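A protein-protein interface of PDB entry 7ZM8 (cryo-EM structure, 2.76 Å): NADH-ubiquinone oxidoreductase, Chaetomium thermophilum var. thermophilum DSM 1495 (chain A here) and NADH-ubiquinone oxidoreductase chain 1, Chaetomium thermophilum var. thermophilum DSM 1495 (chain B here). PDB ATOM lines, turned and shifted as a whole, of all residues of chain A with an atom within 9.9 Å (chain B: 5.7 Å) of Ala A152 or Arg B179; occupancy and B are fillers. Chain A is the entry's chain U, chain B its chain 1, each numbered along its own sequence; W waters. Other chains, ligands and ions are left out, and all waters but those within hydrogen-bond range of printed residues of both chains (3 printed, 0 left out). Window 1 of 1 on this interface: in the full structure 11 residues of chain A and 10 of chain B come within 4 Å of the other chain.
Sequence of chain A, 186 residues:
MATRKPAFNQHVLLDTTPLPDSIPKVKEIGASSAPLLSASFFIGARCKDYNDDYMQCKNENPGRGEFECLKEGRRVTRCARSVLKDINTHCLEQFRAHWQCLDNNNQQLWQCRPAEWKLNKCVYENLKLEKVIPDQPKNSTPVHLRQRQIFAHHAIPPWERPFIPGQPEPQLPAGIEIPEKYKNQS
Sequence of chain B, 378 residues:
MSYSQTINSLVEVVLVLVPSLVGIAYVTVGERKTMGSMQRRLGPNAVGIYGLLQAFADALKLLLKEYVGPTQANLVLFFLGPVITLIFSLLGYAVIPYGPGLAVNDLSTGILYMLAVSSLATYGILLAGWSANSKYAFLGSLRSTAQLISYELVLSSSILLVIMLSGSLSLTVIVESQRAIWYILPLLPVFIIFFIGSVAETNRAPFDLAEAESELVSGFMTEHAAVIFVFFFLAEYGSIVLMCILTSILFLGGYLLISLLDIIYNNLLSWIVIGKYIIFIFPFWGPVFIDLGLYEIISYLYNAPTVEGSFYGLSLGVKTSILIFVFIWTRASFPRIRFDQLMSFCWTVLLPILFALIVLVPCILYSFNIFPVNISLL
A ring nitrogen (NE2) of His A153 sits at hydrogen-bond distance from the side-chain carboxylate (OE2) of Glu B176. NH2 of Arg B179 sits close to NE2 of His A153, at 3.5 Å.
The guanidinium group (NE) of Arg B179 lies within salt-bridge range of the side-chain carboxylate (OE2) of Glu B176 (3.4 Å). OH of Tyr B255 is in hydrogen-bond range of OE1 of Glu B176, at 3.2 Å. The side-chain hydroxyl of Tyr B312 sits at hydrogen-bond distance from the guanidinium group of Arg B179 (3.3 Å). NE1 of Trp A110 lies within hydrogen-bond range of O of Phe A151 (3.3 Å). OE1 of Gln A111 lies within hydrogen-bond range of N of His A153, 2.8 Å away.
Among the printed residues, merely in contact across the chains: Ile A150 with Arg B179 (3.9 Å), Ile A150 with Ala B180 (3.7 Å), Phe A151 with Glu B176 (3.5 Å), Phe A151 with Ser B177 (3.6 Å), Phe A151 with Arg B179 (3.6 Å), Phe A151 with Ala B180 (3.9 Å), Ala A152 with Arg B179 (3.95 Å) and His A153 with Pro B100 (3.7 Å).
Ala A152 touches just one residue of chain B: Arg B179 (3.95 Å). Arg B179 touches just these residues of chain A: Ile A150 (3.9 Å), Phe A151 (3.6 Å), Ala A152 (3.95 Å) and His A153 (3.4 Å). Glu B176 touches just these residues of chain A: Phe A151 and His A153. Printed residues of chain A within 4 Å of Ala B180: Ile A150 (3.7 Å) and Phe A151 (3.9 Å). Of the printed residues of chain B, Ile A150 touches Arg B179 and Ala B180. Printed residues of chain A within 4 Å of Pro B100: His A153 (3.7 Å). Of the printed residues of chain B, His A153 touches Pro B100, Glu B176 and Arg B179. Of the printed residues of chain B, Phe A151 touches Glu B176 (3.5 Å), Ser B177 (3.6 Å), Arg B179 (3.6 Å) and Ala B180 (3.9 Å). Gln A147 touches none of the printed residues of chain B. The nearest printed residue of chain B that does not touch Ala A152 is Glu B176 (7.0 Å). The nearest residue of chain A that does not touch Arg B179 is His A154 (5.6 Å). The nearest printed residue of chain B that does not touch His A153 is Tyr B312 (4.1 Å).
Of the 22 printed residues of chain A, 4 touch a printed residue of chain B. Printed residues of chain A that touch a printed residue of chain B: Ile A150, Phe A151, Ala A152 and His A153. Of the 11 printed residues of chain B, 5 touch a printed residue of chain A. Hydrophobic or aromatic side chains of chain B that line the printed part of chain A: Pro B100 and Ala B180. Among the printed residues, no Asp or Glu carboxylate lies within 4 Å of a Lys or Arg side-chain nitrogen of the other chain.
Water W3 lies within hydrogen-bond range of the side-chain carboxylate (OE2) of Glu B176 (2.7 Å), the backbone carbonyl oxygen (O) of Phe A151 (2.9 Å) and a ring nitrogen (NE2) of His A153 (3.3 Å). Water W1 lies within hydrogen-bond range of the side-chain amide oxygen (OE1) of Gln A108 and the side-chain carboxylate (OE2) of Glu B176. Water W2 bridges NH1 of Arg B179 (3.2 Å) and O of Ala A152 (3.4 Å).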
ATOM      1  N   ASN A 105      18.186   9.700  14.021  1.00  0.00           N
ATOM      2  CA  ASN A 105      19.324  10.065  14.893  1.00  0.00           C
ATOM      3  C   ASN A 105      18.862  10.400  16.311  1.00  0.00           C
ATOM      4  O   ASN A 105      19.575  11.171  16.955  1.00  0.00           O
ATOM      5  CB  ASN A 105      20.185  11.128  14.222  1.00  0.00           C
ATOM      6  CG  ASN A 105      21.045  10.542  13.123  1.00  0.00           C
ATOM      7  OD1 ASN A 105      22.060   9.906  13.394  1.00  0.00           O
ATOM      8  ND2 ASN A 105      20.644  10.735  11.880  1.00  0.00           N
ATOM      9  N   GLN A 108      18.581  14.117  17.590  1.00  0.00           N
ATOM     10  CA  GLN A 108      19.733  14.772  18.280  1.00  0.00           C
ATOM     11  C   GLN A 108      20.467  15.646  17.263  1.00  0.00           C
ATOM     12  O   GLN A 108      20.955  15.084  16.283  1.00  0.00           O
ATOM     13  CB  GLN A 108      20.618  13.748  18.986  1.00  0.00           C
ATOM     14  CG  GLN A 108      19.918  13.003  20.111  1.00  0.00           C
ATOM     15  CD  GLN A 108      20.771  11.891  20.664  1.00  0.00           C
ATOM     16  OE1 GLN A 108      21.736  11.462  20.044  1.00  0.00           O
ATOM     17  NE2 GLN A 108      20.422  11.414  21.846  1.00  0.00           N
ATOM     18  N   LEU A 109      20.538  16.962  17.477  1.00  0.00           N
ATOM     19  CA  LEU A 109      21.083  17.900  16.467  1.00  0.00           C
ATOM     20  C   LEU A 109      22.544  17.614  16.106  1.00  0.00           C
ATOM     21  O   LEU A 109      22.891  17.745  14.941  1.00  0.00           O
ATOM     22  CB  LEU A 109      20.857  19.319  16.994  1.00  0.00           C
ATOM     23  CG  LEU A 109      19.397  19.742  17.133  1.00  0.00           C
ATOM     24  CD1 LEU A 109      19.252  20.872  18.142  1.00  0.00           C
ATOM     25  CD2 LEU A 109      18.824  20.147  15.784  1.00  0.00           C
ATOM     26  N   TRP A 110      23.367  17.231  17.070  1.00  0.00           N
ATOM     27  CA  TRP A 110      24.808  17.015  16.814  1.00  0.00           C
ATOM     28  C   TRP A 110      24.992  15.866  15.822  1.00  0.00           C
ATOM     29  O   TRP A 110      26.064  15.796  15.198  1.00  0.00           O
ATOM     30  CB  TRP A 110      25.551  16.802  18.135  1.00  0.00           C
ATOM     31  CG  TRP A 110      25.128  15.637  18.974  1.00  0.00           C
ATOM     32  CD1 TRP A 110      25.626  14.370  18.934  1.00  0.00           C
ATOM     33  CD2 TRP A 110      24.164  15.655  20.039  1.00  0.00           C
ATOM     34  NE1 TRP A 110      25.018  13.592  19.880  1.00  0.00           N
ATOM     35  CE2 TRP A 110      24.118  14.352  20.576  1.00  0.00           C
ATOM     36  CE3 TRP A 110      23.327  16.635  20.581  1.00  0.00           C
ATOM     37  CZ2 TRP A 110      23.275  14.012  21.629  1.00  0.00           C
ATOM     38  CZ3 TRP A 110      22.492  16.297  21.621  1.00  0.00           C
ATOM     39  CH2 TRP A 110      22.464  15.002  22.132  1.00  0.00           C
ATOM     40  N   GLN A 111      24.008  14.973  15.721  1.00  0.00           N
ATOM     41  CA  GLN A 111      24.089  13.811  14.803  1.00  0.00           C
ATOM     42  C   GLN A 111      23.840  14.200  13.344  1.00  0.00           C
ATOM     43  O   GLN A 111      24.080  13.344  12.489  1.00  0.00           O
ATOM     44  CB  GLN A 111      23.101  12.739  15.238  1.00  0.00           C
ATOM     45  CG  GLN A 111      23.150  12.414  16.720  1.00  0.00           C
ATOM     46  CD  GLN A 111      24.228  11.418  17.063  1.00  0.00           C
ATOM     47  OE1 GLN A 111      25.204  11.257  16.340  1.00  0.00           O
ATOM     48  NE2 GLN A 111      24.056  10.740  18.184  1.00  0.00           N
ATOM     49  N   CYS A 112      23.356  15.406  13.067  1.00  0.00           N
ATOM     50  CA  CYS A 112      22.963  15.749  11.680  1.00  0.00           C
ATOM     51  C   CYS A 112      23.508  17.115  11.288  1.00  0.00           C
ATOM     52  O   CYS A 112      22.785  17.869  10.626  1.00  0.00           O
ATOM     53  CB  CYS A 112      21.446  15.753  11.574  1.00  0.00           C
ATOM     54  SG  CYS A 112      20.700  14.111  11.729  1.00  0.00           S
ATOM     55  N   ARG A 113      24.753  17.404  11.646  1.00  0.00           N
ATOM     56  CA  ARG A 113      25.337  18.752  11.384  1.00  0.00           C
ATOM     57  C   ARG A 113      25.409  19.058   9.891  1.00  0.00           C
ATOM     58  O   ARG A 113      24.968  20.140   9.519  1.00  0.00           O
ATOM     59  CB  ARG A 113      26.677  18.919  12.107  1.00  0.00           C
ATOM     60  CG  ARG A 113      26.567  18.936  13.620  1.00  0.00           C
ATOM     61  CD  ARG A 113      25.729  20.090  14.119  1.00  0.00           C
ATOM     62  NE  ARG A 113      25.943  20.237  15.546  1.00  0.00           N
ATOM     63  CZ  ARG A 113      25.124  20.871  16.365  1.00  0.00           C
ATOM     64  NH1 ARG A 113      25.414  20.948  17.651  1.00  0.00           N
ATOM     65  NH2 ARG A 113      24.021  21.425  15.902  1.00  0.00           N
ATOM     66  N   PRO A 114      25.867  18.159   9.001  1.00  0.00           N
ATOM     67  CA  PRO A 114      26.005  18.520   7.595  1.00  0.00           C
ATOM     68  C   PRO A 114      24.691  18.972   6.950  1.00  0.00           C
ATOM     69  O   PRO A 114      24.718  19.961   6.264  1.00  0.00           O
ATOM     70  CB  PRO A 114      26.486  17.204   6.983  1.00  0.00           C
ATOM     71  CG  PRO A 114      27.294  16.573   8.072  1.00  0.00           C
ATOM     72  CD  PRO A 114      26.438  16.835   9.285  1.00  0.00           C
ATOM     73  N   TRP A 117      23.740  22.495   8.287  1.00  0.00           N
ATOM     74  CA  TRP A 117      24.623  23.552   7.752  1.00  0.00           C
ATOM     75  C   TRP A 117      24.141  23.964   6.361  1.00  0.00           C
ATOM     76  O   TRP A 117      24.228  25.151   6.048  1.00  0.00           O
ATOM     77  CB  TRP A 117      26.072  23.062   7.748  1.00  0.00           C
ATOM     78  CG  TRP A 117      26.700  22.893   9.094  1.00  0.00           C
ATOM     79  CD1 TRP A 117      26.378  23.540  10.250  1.00  0.00           C
ATOM     80  CD2 TRP A 117      27.801  22.027   9.414  1.00  0.00           C
ATOM     81  NE1 TRP A 117      27.191  23.123  11.268  1.00  0.00           N
ATOM     82  CE2 TRP A 117      28.077  22.199  10.786  1.00  0.00           C
ATOM     83  CE3 TRP A 117      28.576  21.126   8.679  1.00  0.00           C
ATOM     84  CZ2 TRP A 117      29.096  21.504  11.434  1.00  0.00           C
ATOM     85  CZ3 TRP A 117      29.579  20.439   9.321  1.00  0.00           C
ATOM     86  CH2 TRP A 117      29.837  20.628  10.678  1.00  0.00           C
ATOM     87  N   VAL A 143      29.196  25.267  19.640  1.00  0.00           N
ATOM     88  CA  VAL A 143      29.135  23.789  19.461  1.00  0.00           C
ATOM     89  C   VAL A 143      28.497  23.434  18.114  1.00  0.00           C
ATOM     90  O   VAL A 143      28.874  22.408  17.547  1.00  0.00           O
ATOM     91  CB  VAL A 143      28.420  23.131  20.665  1.00  0.00           C
ATOM     92  CG1 VAL A 143      26.906  23.261  20.602  1.00  0.00           C
ATOM     93  CG2 VAL A 143      28.831  21.679  20.853  1.00  0.00           C
ATOM     94  N   ARG A 146      31.050  23.746  15.074  1.00  0.00           N
ATOM     95  CA  ARG A 146      32.330  23.002  15.226  1.00  0.00           C
ATOM     96  C   ARG A 146      32.471  21.935  14.149  1.00  0.00           C
ATOM     97  O   ARG A 146      31.505  21.199  13.941  1.00  0.00           O
ATOM     98  CB  ARG A 146      32.405  22.294  16.579  1.00  0.00           C
ATOM     99  CG  ARG A 146      32.623  23.221  17.760  1.00  0.00           C
ATOM    100  CD  ARG A 146      32.665  22.563  19.119  1.00  0.00           C
ATOM    101  NE  ARG A 146      32.811  23.624  20.102  1.00  0.00           N
ATOM    102  CZ  ARG A 146      32.806  23.458  21.417  1.00  0.00           C
ATOM    103  NH1 ARG A 146      32.944  24.505  22.208  1.00  0.00           N
ATOM    104  NH2 ARG A 146      32.666  22.253  21.935  1.00  0.00           N
ATOM    105  N   GLN A 147      33.656  21.819  13.553  1.00  0.00           N
ATOM    106  CA  GLN A 147      33.925  20.821  12.495  1.00  0.00           C
ATOM    107  C   GLN A 147      33.822  19.411  13.080  1.00  0.00           C
ATOM    108  O   GLN A 147      33.372  18.500  12.369  1.00  0.00           O
ATOM    109  CB  GLN A 147      35.280  21.093  11.856  1.00  0.00           C
ATOM    110  CG  GLN A 147      35.641  20.119  10.744  1.00  0.00           C
ATOM    111  CD  GLN A 147      34.669  20.182   9.593  1.00  0.00           C
ATOM    112  OE1 GLN A 147      34.219  21.252   9.201  1.00  0.00           O
ATOM    113  NE2 GLN A 147      34.350  19.030   9.030  1.00  0.00           N
ATOM    114  N   ARG A 148      34.252  19.240  14.327  1.00  0.00           N
ATOM    115  CA  ARG A 148      34.183  17.913  14.916  1.00  0.00           C
ATOM    116  C   ARG A 148      33.129  17.893  16.011  1.00  0.00           C
ATOM    117  O   ARG A 148      33.055  18.818  16.825  1.00  0.00           O
ATOM    118  CB  ARG A 148      35.540  17.497  15.480  1.00  0.00           C
ATOM    119  CG  ARG A 148      36.613  17.302  14.426  1.00  0.00           C
ATOM    120  CD  ARG A 148      37.934  16.913  15.062  1.00  0.00           C
ATOM    121  NE  ARG A 148      37.852  15.594  15.683  1.00  0.00           N
ATOM    122  CZ  ARG A 148      38.799  15.065  16.450  1.00  0.00           C
ATOM    123  NH1 ARG A 148      38.635  13.857  16.971  1.00  0.00           N
ATOM    124  NH2 ARG A 148      39.910  15.745  16.697  1.00  0.00           N
ATOM    125  N   GLN A 149      32.307  16.840  16.016  1.00  0.00           N
ATOM    126  CA  GLN A 149      31.338  16.640  17.119  1.00  0.00           C
ATOM    127  C   GLN A 149      31.739  15.342  17.803  1.00  0.00           C
ATOM    128  O   GLN A 149      31.712  14.302  17.144  1.00  0.00           O
ATOM    129  CB  GLN A 149      29.902  16.547  16.596  1.00  0.00           C
ATOM    130  CG  GLN A 149      29.396  17.804  15.909  1.00  0.00           C
ATOM    131  CD  GLN A 149      29.212  18.978  16.839  1.00  0.00           C
ATOM    132  OE1 GLN A 149      28.879  18.829  18.010  1.00  0.00           O
ATOM    133  NE2 GLN A 149      29.410  20.170  16.305  1.00  0.00           N
ATOM    134  N   ILE A 150      32.144  15.430  19.067  1.00  0.00           N
ATOM    135  CA  ILE A 150      32.658  14.243  19.803  1.00  0.00           C
ATOM    136  C   ILE A 150      31.550  13.209  19.975  1.00  0.00           C
ATOM    137  O   ILE A 150      31.826  12.019  19.790  1.00  0.00           O
ATOM    138  CB  ILE A 150      33.201  14.716  21.170  1.00  0.00           C
ATOM    139  CG1 ILE A 150      34.568  15.389  21.048  1.00  0.00           C
ATOM    140  CG2 ILE A 150      33.216  13.594  22.194  1.00  0.00           C
ATOM    141  CD1 ILE A 150      35.045  16.031  22.333  1.00  0.00           C
ATOM    142  N   PHE A 151      30.338  13.655  20.306  1.00  0.00           N
ATOM    143  CA  PHE A 151      29.274  12.690  20.656  1.00  0.00           C
ATOM    144  C   PHE A 151      28.518  12.225  19.421  1.00  0.00           C
ATOM    145  O   PHE A 151      27.558  11.456  19.569  1.00  0.00           O
ATOM    146  CB  PHE A 151      28.441  13.239  21.812  1.00  0.00           C
ATOM    147  CG  PHE A 151      29.239  13.494  23.061  1.00  0.00           C
ATOM    148  CD1 PHE A 151      29.555  12.456  23.921  1.00  0.00           C
ATOM    149  CD2 PHE A 151      29.692  14.767  23.367  1.00  0.00           C
ATOM    150  CE1 PHE A 151      30.298  12.687  25.066  1.00  0.00           C
ATOM    151  CE2 PHE A 151      30.437  14.994  24.510  1.00  0.00           C
ATOM    152  CZ  PHE A 151      30.738  13.954  25.357  1.00  0.00           C
ATOM    153  N   ALA A 152      28.964  12.658  18.241  1.00  0.00           N
ATOM    154  CA  ALA A 152      28.342  12.175  16.981  1.00  0.00           C
ATOM    155  C   ALA A 152      28.644  10.696  16.746  1.00  0.00           C
ATOM    156  O   ALA A 152      29.806  10.305  16.886  1.00  0.00           O
ATOM    157  CB  ALA A 152      28.805  12.995  15.816  1.00  0.00           C
ATOM    158  N   HIS A 153      27.625   9.913  16.399  1.00  0.00           N
ATOM    159  CA  HIS A 153      27.782   8.467  16.091  1.00  0.00           C
ATOM    160  C   HIS A 153      28.614   8.295  14.829  1.00  0.00           C
ATOM    161  O   HIS A 153      29.403   7.346  14.782  1.00  0.00           O
ATOM    162  CB  HIS A 153      26.418   7.794  15.962  1.00  0.00           C
ATOM    163  CG  HIS A 153      25.672   7.668  17.246  1.00  0.00           C
ATOM    164  ND1 HIS A 153      24.730   6.686  17.457  1.00  0.00           N
ATOM    165  CD2 HIS A 153      25.723   8.392  18.383  1.00  0.00           C
ATOM    166  CE1 HIS A 153      24.232   6.811  18.668  1.00  0.00           C
ATOM    167  NE2 HIS A 153      24.822   7.852  19.254  1.00  0.00           N
ATOM    168  N   HIS A 154      28.435   9.187  13.856  1.00  0.00           N
ATOM    169  CA  HIS A 154      29.214   9.134  12.595  1.00  0.00           C
ATOM    170  C   HIS A 154      30.091  10.377  12.482  1.00  0.00           C
ATOM    171  O   HIS A 154      29.604  11.470  12.802  1.00  0.00           O
ATOM    172  CB  HIS A 154      28.273   8.981  11.399  1.00  0.00           C
ATOM    173  CG  HIS A 154      27.323   7.845  11.562  1.00  0.00           C
ATOM    174  ND1 HIS A 154      27.735   6.529  11.497  1.00  0.00           N
ATOM    175  CD2 HIS A 154      25.996   7.818  11.810  1.00  0.00           C
ATOM    176  CE1 HIS A 154      26.699   5.739  11.689  1.00  0.00           C
ATOM    177  NE2 HIS A 154      25.619   6.504  11.884  1.00  0.00           N
ATOM    178  N   ALA A 155      31.330  10.208  12.016  1.00  0.00           N
ATOM    179  CA  ALA A 155      32.248  11.324  11.844  1.00  0.00           C
ATOM    180  C   ALA A 155      31.734  12.297  10.794  1.00  0.00           C
ATOM    181  O   ALA A 155      31.155  11.897   9.782  1.00  0.00           O
ATOM    182  CB  ALA A 155      33.630  10.814  11.447  1.00  0.00           C
ATOM    183  N   ILE A 156      31.950  13.583  11.046  1.00  0.00           N
ATOM    184  CA  ILE A 156      31.594  14.628  10.092  1.00  0.00           C
ATOM    185  C   ILE A 156      32.696  14.731   9.049  1.00  0.00           C
ATOM    186  O   ILE A 156      33.866  14.922   9.406  1.00  0.00           O
ATOM    187  CB  ILE A 156      31.368  15.976  10.790  1.00  0.00           C
ATOM    188  CG1 ILE A 156      30.132  15.911  11.685  1.00  0.00           C
ATOM    189  CG2 ILE A 156      31.226  17.077   9.764  1.00  0.00           C
ATOM    190  CD1 ILE A 156      29.944  17.130  12.531  1.00  0.00           C
ATOM    191  N   PRO A 157      32.378  14.594   7.768  1.00  0.00           N
ATOM    192  CA  PRO A 157      33.400  14.659   6.729  1.00  0.00           C
ATOM    193  C   PRO A 157      34.078  16.015   6.707  1.00  0.00           C
ATOM    194  O   PRO A 157      33.427  17.048   6.912  1.00  0.00           O
ATOM    195  CB  PRO A 157      32.603  14.417   5.443  1.00  0.00           C
ATOM    196  CG  PRO A 157      31.394  13.706   5.881  1.00  0.00           C
ATOM    197  CD  PRO A 157      31.054  14.289   7.206  1.00  0.00           C
ATOM    198  N   PRO B 100      22.628   1.681  21.320  1.00  0.00           N
ATOM    199  CA  PRO B 100      21.934   2.786  21.993  1.00  0.00           C
ATOM    200  C   PRO B 100      20.472   2.486  22.281  1.00  0.00           C
ATOM    201  O   PRO B 100      19.642   2.408  21.374  1.00  0.00           O
ATOM    202  CB  PRO B 100      22.089   3.939  21.000  1.00  0.00           C
ATOM    203  CG  PRO B 100      23.367   3.646  20.326  1.00  0.00           C
ATOM    204  CD  PRO B 100      23.439   2.152  20.190  1.00  0.00           C
ATOM    205  N   VAL B 175      27.337   4.731  28.674  1.00  0.00           N
ATOM    206  CA  VAL B 175      28.210   4.366  27.521  1.00  0.00           C
ATOM    207  C   VAL B 175      28.359   5.559  26.576  1.00  0.00           C
ATOM    208  O   VAL B 175      29.487   5.818  26.148  1.00  0.00           O
ATOM    209  CB  VAL B 175      27.722   3.096  26.792  1.00  0.00           C
ATOM    210  CG1 VAL B 175      28.444   2.872  25.477  1.00  0.00           C
ATOM    211  CG2 VAL B 175      27.832   1.870  27.677  1.00  0.00           C
ATOM    212  N   GLU B 176      27.278   6.259  26.268  1.00  0.00           N
ATOM    213  CA  GLU B 176      27.313   7.377  25.290  1.00  0.00           C
ATOM    214  C   GLU B 176      28.237   8.493  25.764  1.00  0.00           C
ATOM    215  O   GLU B 176      28.731   9.214  24.908  1.00  0.00           O
ATOM    216  CB  GLU B 176      25.883   7.867  25.081  1.00  0.00           C
ATOM    217  CG  GLU B 176      25.026   6.875  24.324  1.00  0.00           C
ATOM    218  CD  GLU B 176      25.484   6.657  22.897  1.00  0.00           C
ATOM    219  OE1 GLU B 176      26.043   5.587  22.603  1.00  0.00           O
ATOM    220  OE2 GLU B 176      25.287   7.568  22.090  1.00  0.00           O
ATOM    221  N   SER B 177      28.360   8.688  27.073  1.00  0.00           N
ATOM    222  CA  SER B 177      29.254   9.693  27.685  1.00  0.00           C
ATOM    223  C   SER B 177      30.701   9.334  27.380  1.00  0.00           C
ATOM    224  O   SER B 177      31.537  10.236  27.322  1.00  0.00           O
ATOM    225  CB  SER B 177      28.981   9.750  29.139  1.00  0.00           C
ATOM    226  OG  SER B 177      27.623  10.067  29.377  1.00  0.00           O
ATOM    227  N   GLN B 178      30.974   8.048  27.246  1.00  0.00           N
ATOM    228  CA  GLN B 178      32.341   7.549  26.988  1.00  0.00           C
ATOM    229  C   GLN B 178      32.785   7.786  25.544  1.00  0.00           C
ATOM    230  O   GLN B 178      33.870   7.311  25.199  1.00  0.00           O
ATOM    231  CB  GLN B 178      32.464   6.133  27.524  1.00  0.00           C
ATOM    232  CG  GLN B 178      32.077   6.035  28.986  1.00  0.00           C
ATOM    233  CD  GLN B 178      32.413   4.689  29.567  1.00  0.00           C
ATOM    234  OE1 GLN B 178      33.567   4.283  29.591  1.00  0.00           O
ATOM    235  NE2 GLN B 178      31.400   4.001  30.058  1.00  0.00           N
ATOM    236  N   ARG B 179      31.993   8.492  24.741  1.00  0.00           N
ATOM    237  CA  ARG B 179      32.436   8.865  23.378  1.00  0.00           C
ATOM    238  C   ARG B 179      33.587   9.861  23.532  1.00  0.00           C
ATOM    239  O   ARG B 179      34.424   9.919  22.627  1.00  0.00           O
ATOM    240  CB  ARG B 179      31.260   9.350  22.536  1.00  0.00           C
ATOM    241  CG  ARG B 179      30.373   8.233  22.006  1.00  0.00           C
ATOM    242  CD  ARG B 179      29.276   8.683  21.063  1.00  0.00           C
ATOM    243  NE  ARG B 179      28.369   7.585  20.765  1.00  0.00           N
ATOM    244  CZ  ARG B 179      28.483   6.762  19.730  1.00  0.00           C
ATOM    245  NH1 ARG B 179      29.473   6.901  18.866  1.00  0.00           N
ATOM    246  NH2 ARG B 179      27.606   5.788  19.565  1.00  0.00           N
ATOM    247  N   ALA B 180      33.578  10.662  24.596  1.00  0.00           N
ATOM    248  CA  ALA B 180      34.705  11.573  24.886  1.00  0.00           C
ATOM    249  C   ALA B 180      35.964  10.801  25.266  1.00  0.00           C
ATOM    250  O   ALA B 180      37.029  11.128  24.726  1.00  0.00           O
ATOM    251  CB  ALA B 180      34.305  12.483  26.010  1.00  0.00           C
ATOM    252  N   ILE B 181      35.837   9.808  26.139  1.00  0.00           N
ATOM    253  CA  ILE B 181      36.999   9.013  26.628  1.00  0.00           C
ATOM    254  C   ILE B 181      36.427   7.810  27.367  1.00  0.00           C
ATOM    255  O   ILE B 181      35.362   7.957  27.972  1.00  0.00           O
ATOM    256  CB  ILE B 181      37.915   9.850  27.549  1.00  0.00           C
ATOM    257  CG1 ILE B 181      39.246   9.148  27.825  1.00  0.00           C
ATOM    258  CG2 ILE B 181      37.218  10.267  28.835  1.00  0.00           C
ATOM    259  CD1 ILE B 181      40.071   8.907  26.591  1.00  0.00           C
ATOM    260  N   TYR B 255      29.606  -0.588  24.177  1.00  0.00           N
ATOM    261  CA  TYR B 255      29.484  -1.105  22.793  1.00  0.00           C
ATOM    262  C   TYR B 255      30.221  -0.174  21.839  1.00  0.00           C
ATOM    263  O   TYR B 255      30.170  -0.389  20.625  1.00  0.00           O
ATOM    264  CB  TYR B 255      28.011  -1.216  22.396  1.00  0.00           C
ATOM    265  CG  TYR B 255      27.130  -0.065  22.813  1.00  0.00           C
ATOM    266  CD1 TYR B 255      27.108   1.121  22.098  1.00  0.00           C
ATOM    267  CD2 TYR B 255      26.298  -0.171  23.914  1.00  0.00           C
ATOM    268  CE1 TYR B 255      26.303   2.180  22.481  1.00  0.00           C
ATOM    269  CE2 TYR B 255      25.481   0.874  24.307  1.00  0.00           C
ATOM    270  CZ  TYR B 255      25.482   2.054  23.588  1.00  0.00           C
ATOM    271  OH  TYR B 255      24.677   3.084  23.973  1.00  0.00           O
ATOM    272  N   LEU B 256      30.911   0.823  22.385  1.00  0.00           N
ATOM    273  CA  LEU B 256      31.604   1.827  21.538  1.00  0.00           C
ATOM    274  C   LEU B 256      32.858   1.220  20.922  1.00  0.00           C
ATOM    275  O   LEU B 256      33.705   0.745  21.672  1.00  0.00           O
ATOM    276  CB  LEU B 256      31.968   3.035  22.396  1.00  0.00           C
ATOM    277  CG  LEU B 256      30.799   3.924  22.795  1.00  0.00           C
ATOM    278  CD1 LEU B 256      31.304   5.157  23.516  1.00  0.00           C
ATOM    279  CD2 LEU B 256      29.991   4.310  21.572  1.00  0.00           C
ATOM    280  N   TYR B 312      28.152  -3.394  17.108  1.00  0.00           N
ATOM    281  CA  TYR B 312      28.039  -2.822  18.472  1.00  0.00           C
ATOM    282  C   TYR B 312      28.012  -4.001  19.443  1.00  0.00           C
ATOM    283  O   TYR B 312      28.629  -3.910  20.519  1.00  0.00           O
ATOM    284  CB  TYR B 312      26.790  -1.945  18.595  1.00  0.00           C
ATOM    285  CG  TYR B 312      26.942  -0.500  18.199  1.00  0.00           C
ATOM    286  CD1 TYR B 312      28.166   0.142  18.270  1.00  0.00           C
ATOM    287  CD2 TYR B 312      25.849   0.244  17.784  1.00  0.00           C
ATOM    288  CE1 TYR B 312      28.306   1.476  17.922  1.00  0.00           C
ATOM    289  CE2 TYR B 312      25.970   1.577  17.430  1.00  0.00           C
ATOM    290  CZ  TYR B 312      27.204   2.196  17.500  1.00  0.00           C
ATOM    291  OH  TYR B 312      27.337   3.510  17.153  1.00  0.00           O
HETATM  292  O   HOH W   1      23.021   9.690  22.160  1.00  0.00           O
HETATM  293  O   HOH W   2      32.129   8.646  18.815  1.00  0.00           O
HETATM  294  O   HOH W   3      25.592  10.205  21.373  1.00  0.00           O
